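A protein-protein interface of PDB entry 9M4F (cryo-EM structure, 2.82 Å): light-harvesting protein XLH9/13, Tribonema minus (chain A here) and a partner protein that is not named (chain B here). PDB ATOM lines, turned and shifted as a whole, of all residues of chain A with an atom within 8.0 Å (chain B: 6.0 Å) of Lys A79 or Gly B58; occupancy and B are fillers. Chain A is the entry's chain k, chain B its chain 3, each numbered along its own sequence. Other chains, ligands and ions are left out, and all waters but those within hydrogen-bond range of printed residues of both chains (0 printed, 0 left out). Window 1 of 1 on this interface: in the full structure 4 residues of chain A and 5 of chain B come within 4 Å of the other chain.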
ATOM      1  N   PRO A  73       1.957  18.821  14.827  1.00  0.00           N
ATOM      2  CA  PRO A  73       2.945  19.776  14.293  1.00  0.00           C
ATOM      3  C   PRO A  73       3.445  19.393  12.912  1.00  0.00           C
ATOM      4  O   PRO A  73       3.395  20.212  11.985  1.00  0.00           O
ATOM      5  CB  PRO A  73       4.066  19.744  15.344  1.00  0.00           C
ATOM      6  CG  PRO A  73       3.442  19.195  16.569  1.00  0.00           C
ATOM      7  CD  PRO A  73       2.389  18.247  16.114  1.00  0.00           C
ATOM      8  N   LEU A  74       3.924  18.160  12.746  1.00  0.00           N
ATOM      9  CA  LEU A  74       4.331  17.702  11.425  1.00  0.00           C
ATOM     10  C   LEU A  74       3.160  17.678  10.454  1.00  0.00           C
ATOM     11  O   LEU A  74       3.377  17.694   9.237  1.00  0.00           O
ATOM     12  CB  LEU A  74       4.964  16.311  11.521  1.00  0.00           C
ATOM     13  CG  LEU A  74       6.068  16.133  12.567  1.00  0.00           C
ATOM     14  CD1 LEU A  74       6.724  14.768  12.420  1.00  0.00           C
ATOM     15  CD2 LEU A  74       7.110  17.234  12.472  1.00  0.00           C
ATOM     16  N   GLY A  75       1.931  17.642  10.961  1.00  0.00           N
ATOM     17  CA  GLY A  75       0.763  17.653  10.094  1.00  0.00           C
ATOM     18  C   GLY A  75       0.686  16.451   9.180  1.00  0.00           C
ATOM     19  O   GLY A  75       0.340  16.591   8.000  1.00  0.00           O
ATOM     20  N   LEU A  76       1.005  15.265   9.700  1.00  0.00           N
ATOM     21  CA  LEU A  76       1.011  14.070   8.865  1.00  0.00           C
ATOM     22  C   LEU A  76      -0.396  13.721   8.388  1.00  0.00           C
ATOM     23  O   LEU A  76      -0.587  13.329   7.231  1.00  0.00           O
ATOM     24  CB  LEU A  76       1.629  12.904   9.635  1.00  0.00           C
ATOM     25  CG  LEU A  76       2.973  13.207  10.307  1.00  0.00           C
ATOM     26  CD1 LEU A  76       3.494  11.988  11.048  1.00  0.00           C
ATOM     27  CD2 LEU A  76       3.997  13.689   9.291  1.00  0.00           C
ATOM     28  N   ALA A  77      -1.397  13.868   9.257  1.00  0.00           N
ATOM     29  CA  ALA A  77      -2.763  13.550   8.858  1.00  0.00           C
ATOM     30  C   ALA A  77      -3.241  14.424   7.711  1.00  0.00           C
ATOM     31  O   ALA A  77      -4.207  14.061   7.031  1.00  0.00           O
ATOM     32  CB  ALA A  77      -3.710  13.698  10.047  1.00  0.00           C
ATOM     33  N   GLU A  78      -2.591  15.564   7.477  1.00  0.00           N
ATOM     34  CA  GLU A  78      -2.952  16.416   6.353  1.00  0.00           C
ATOM     35  C   GLU A  78      -2.674  15.754   5.011  1.00  0.00           C
ATOM     36  O   GLU A  78      -3.145  16.257   3.985  1.00  0.00           O
ATOM     37  CB  GLU A  78      -2.199  17.745   6.440  1.00  0.00           C
ATOM     38  CG  GLU A  78      -2.352  18.452   7.779  1.00  0.00           C
ATOM     39  CD  GLU A  78      -3.804  18.659   8.168  1.00  0.00           C
ATOM     40  OE1 GLU A  78      -4.650  18.811   7.262  1.00  0.00           O
ATOM     41  OE2 GLU A  78      -4.100  18.660   9.381  1.00  0.00           O
ATOM     42  N   LYS A  79      -1.926  14.652   4.991  1.00  0.00           N
ATOM     43  CA  LYS A  79      -1.669  13.916   3.761  1.00  0.00           C
ATOM     44  C   LYS A  79      -2.799  12.956   3.402  1.00  0.00           C
ATOM     45  O   LYS A  79      -2.635  12.144   2.488  1.00  0.00           O
ATOM     46  CB  LYS A  79      -0.349  13.147   3.876  1.00  0.00           C
ATOM     47  CG  LYS A  79       0.782  13.925   4.545  1.00  0.00           C
ATOM     48  CD  LYS A  79       1.106  15.226   3.830  1.00  0.00           C
ATOM     49  CE  LYS A  79       1.392  16.341   4.824  1.00  0.00           C
ATOM     50  NZ  LYS A  79       2.507  16.002   5.751  1.00  0.00           N
ATOM     51  N   GLY A  80      -3.929  13.027   4.102  1.00  0.00           N
ATOM     52  CA  GLY A  80      -5.071  12.190   3.811  1.00  0.00           C
ATOM     53  C   GLY A  80      -4.991  10.832   4.487  1.00  0.00           C
ATOM     54  O   GLY A  80      -3.955  10.408   5.005  1.00  0.00           O
ATOM     55  N   ASP A  81      -6.127  10.135   4.473  1.00  0.00           N
ATOM     56  CA  ASP A  81      -6.234   8.789   5.032  1.00  0.00           C
ATOM     57  C   ASP A  81      -5.841   8.781   6.511  1.00  0.00           C
ATOM     58  O   ASP A  81      -4.857   8.163   6.923  1.00  0.00           O
ATOM     59  CB  ASP A  81      -5.382   7.804   4.227  1.00  0.00           C
ATOM     60  CG  ASP A  81      -5.713   7.824   2.747  1.00  0.00           C
ATOM     61  OD1 ASP A  81      -6.655   8.548   2.359  1.00  0.00           O
ATOM     62  OD2 ASP A  81      -5.030   7.122   1.974  1.00  0.00           O
ATOM     63  N   VAL A  82      -6.637   9.493   7.310  1.00  0.00           N
ATOM     64  CA  VAL A  82      -6.390   9.565   8.746  1.00  0.00           C
ATOM     65  C   VAL A  82      -6.954   8.355   9.480  1.00  0.00           C
ATOM     66  O   VAL A  82      -6.546   8.084  10.616  1.00  0.00           O
ATOM     67  CB  VAL A  82      -6.989  10.851   9.341  1.00  0.00           C
ATOM     68  CG1 VAL A  82      -6.457  11.089  10.745  1.00  0.00           C
ATOM     69  CG2 VAL A  82      -6.693  12.052   8.449  1.00  0.00           C
ATOM     70  N   TYR A  85      -4.284   5.855  10.387  1.00  0.00           N
ATOM     71  CA  TYR A  85      -3.497   6.337  11.515  1.00  0.00           C
ATOM     72  C   TYR A  85      -4.259   6.168  12.820  1.00  0.00           C
ATOM     73  O   TYR A  85      -3.679   5.785  13.843  1.00  0.00           O
ATOM     74  CB  TYR A  85      -3.120   7.804  11.299  1.00  0.00           C
ATOM     75  CG  TYR A  85      -2.159   8.040  10.154  1.00  0.00           C
ATOM     76  CD1 TYR A  85      -2.542   7.815   8.840  1.00  0.00           C
ATOM     77  CD2 TYR A  85      -0.873   8.503  10.388  1.00  0.00           C
ATOM     78  CE1 TYR A  85      -1.670   8.033   7.794  1.00  0.00           C
ATOM     79  CE2 TYR A  85       0.007   8.725   9.349  1.00  0.00           C
ATOM     80  CZ  TYR A  85      -0.397   8.488   8.053  1.00  0.00           C
ATOM     81  OH  TYR A  85       0.473   8.708   7.011  1.00  0.00           O
ATOM     82  N   GLN A 156     -10.997   4.301   3.516  1.00  0.00           N
ATOM     83  CA  GLN A 156     -12.040   5.298   3.317  1.00  0.00           C
ATOM     84  C   GLN A 156     -13.308   4.693   2.734  1.00  0.00           C
ATOM     85  O   GLN A 156     -14.389   5.266   2.905  1.00  0.00           O
ATOM     86  CB  GLN A 156     -11.544   6.423   2.403  1.00  0.00           C
ATOM     87  CG  GLN A 156     -10.447   7.290   3.008  1.00  0.00           C
ATOM     88  CD  GLN A 156     -10.356   8.659   2.355  1.00  0.00           C
ATOM     89  OE1 GLN A 156     -11.163   9.003   1.491  1.00  0.00           O
ATOM     90  NE2 GLN A 156      -9.373   9.449   2.770  1.00  0.00           N
ATOM     91  N   ASP B  55       3.565   8.103   0.073  1.00  0.00           N
ATOM     92  CA  ASP B  55       4.141   9.326   0.630  1.00  0.00           C
ATOM     93  C   ASP B  55       3.521   9.591   1.996  1.00  0.00           C
ATOM     94  O   ASP B  55       2.805  10.580   2.191  1.00  0.00           O
ATOM     95  CB  ASP B  55       3.914  10.504  -0.319  1.00  0.00           C
ATOM     96  CG  ASP B  55       4.829  11.675  -0.032  1.00  0.00           C
ATOM     97  OD1 ASP B  55       5.971  11.443   0.410  1.00  0.00           O
ATOM     98  OD2 ASP B  55       4.405  12.829  -0.246  1.00  0.00           O
ATOM     99  N   PRO B  56       3.777   8.714   2.979  1.00  0.00           N
ATOM    100  CA  PRO B  56       3.245   8.957   4.328  1.00  0.00           C
ATOM    101  C   PRO B  56       3.636  10.321   4.870  1.00  0.00           C
ATOM    102  O   PRO B  56       2.767  11.141   5.180  1.00  0.00           O
ATOM    103  CB  PRO B  56       3.861   7.824   5.156  1.00  0.00           C
ATOM    104  CG  PRO B  56       4.087   6.739   4.186  1.00  0.00           C
ATOM    105  CD  PRO B  56       4.422   7.394   2.878  1.00  0.00           C
ATOM    106  N   LEU B  57       4.935  10.578   4.983  1.00  0.00           N
ATOM    107  CA  LEU B  57       5.409  11.911   5.316  1.00  0.00           C
ATOM    108  C   LEU B  57       5.327  12.789   4.078  1.00  0.00           C
ATOM    109  O   LEU B  57       5.687  12.368   2.976  1.00  0.00           O
ATOM    110  CB  LEU B  57       6.845  11.865   5.836  1.00  0.00           C
ATOM    111  CG  LEU B  57       7.122  10.892   6.985  1.00  0.00           C
ATOM    112  CD1 LEU B  57       8.576  10.985   7.418  1.00  0.00           C
ATOM    113  CD2 LEU B  57       6.199  11.156   8.160  1.00  0.00           C
ATOM    114  N   GLY B  58       4.852  14.016   4.257  1.00  0.00           N
ATOM    115  CA  GLY B  58       4.659  14.879   3.113  1.00  0.00           C
ATOM    116  C   GLY B  58       5.967  15.444   2.606  1.00  0.00           C
ATOM    117  O   GLY B  58       6.533  16.367   3.202  1.00  0.00           O
ATOM    118  N   PHE B  59       6.451  14.899   1.496  1.00  0.00           N
ATOM    119  CA  PHE B  59       7.659  15.375   0.838  1.00  0.00           C
ATOM    120  C   PHE B  59       7.401  15.867  -0.574  1.00  0.00           C
ATOM    121  O   PHE B  59       8.011  16.850  -0.998  1.00  0.00           O
ATOM    122  CB  PHE B  59       8.720  14.265   0.799  1.00  0.00           C
ATOM    123  CG  PHE B  59       9.342  13.958   2.135  1.00  0.00           C
ATOM    124  CD1 PHE B  59       9.643  14.969   3.030  1.00  0.00           C
ATOM    125  CD2 PHE B  59       9.635  12.655   2.489  1.00  0.00           C
ATOM    126  CE1 PHE B  59      10.217  14.682   4.252  1.00  0.00           C
ATOM    127  CE2 PHE B  59      10.211  12.365   3.710  1.00  0.00           C
ATOM    128  CZ  PHE B  59      10.502  13.378   4.590  1.00  0.00           C
ATOM    129  N   ALA B  60       6.516  15.204  -1.317  1.00  0.00           N
ATOM    130  CA  ALA B  60       6.098  15.655  -2.636  1.00  0.00           C
ATOM    131  C   ALA B  60       4.694  16.242  -2.628  1.00  0.00           C
ATOM    132  O   ALA B  60       4.158  16.560  -3.694  1.00  0.00           O
ATOM    133  CB  ALA B  60       6.177  14.500  -3.637  1.00  0.00           C
ATOM    134  N   SER B  61       4.083  16.393  -1.451  1.00  0.00           N
ATOM    135  CA  SER B  61       2.718  16.903  -1.383  1.00  0.00           C
ATOM    136  C   SER B  61       2.637  18.330  -1.913  1.00  0.00           C
ATOM    137  O   SER B  61       1.737  18.666  -2.689  1.00  0.00           O
ATOM    138  CB  SER B  61       2.210  16.835   0.056  1.00  0.00           C
ATOM    139  OG  SER B  61       2.213  15.501   0.531  1.00  0.00           O
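Of the printed residues of chain B, Leu A76 touches Leu B57 (3.5 Å).
Lys A79 touches just these residues of chain B: Pro B56, Gly B58 and Ser B61.
Printed residues of chain A within 4 Å of Pro B56: Lys A79 and Tyr A85.
Of the printed residues of chain A, Leu B57 touches Leu A76 (3.5 Å).
Gly B58 touches just one residue of chain A: Lys A79 (3.4 Å).
Of the printed residues of chain A, Ser B61 touches Lys A79.
The nearest residue of chain B that does not touch Lys A79 is Asp B55 (4.4 Å).
The nearest printed residue of chain A that does not touch Leu B57 is Lys A79 (4.6 Å).
Of the 12 printed residues of chain A, 3 touch a printed residue of chain B.
Of the 7 printed residues of chain B, 4 touch a printed residue of chain A.
Hydrophobic or aromatic side chains of chain B within 4 Å of the printed part of chain A: Pro B56 and Leu B57.
Among the printed residues, no Asp or Glu carboxylate lies within 4 Å of a Lys or Arg side-chain nitrogen of the other chain.
The side-chain carboxylate of Asp B55 lies close to the backbone carbonyl oxygen of Leu B57, 2.7 Å away.
The backbone carbonyl oxygen of Gly A75 sits at hydrogen-bond distance from the side-chain amino group of Lys A79 (3.2 Å).
Among the printed residues, pairs that only touch across the chains: Leu A76 with Leu B57 (3.5 Å), Lys A79 with Pro B56 (3.5 Å), Lys A79 with Ser B61 (3.5 Å) and Tyr A85 with Pro B56 (3.8 Å).
N of Gly B58 sits close to NZ of Lys A79, 3.4 Å away.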
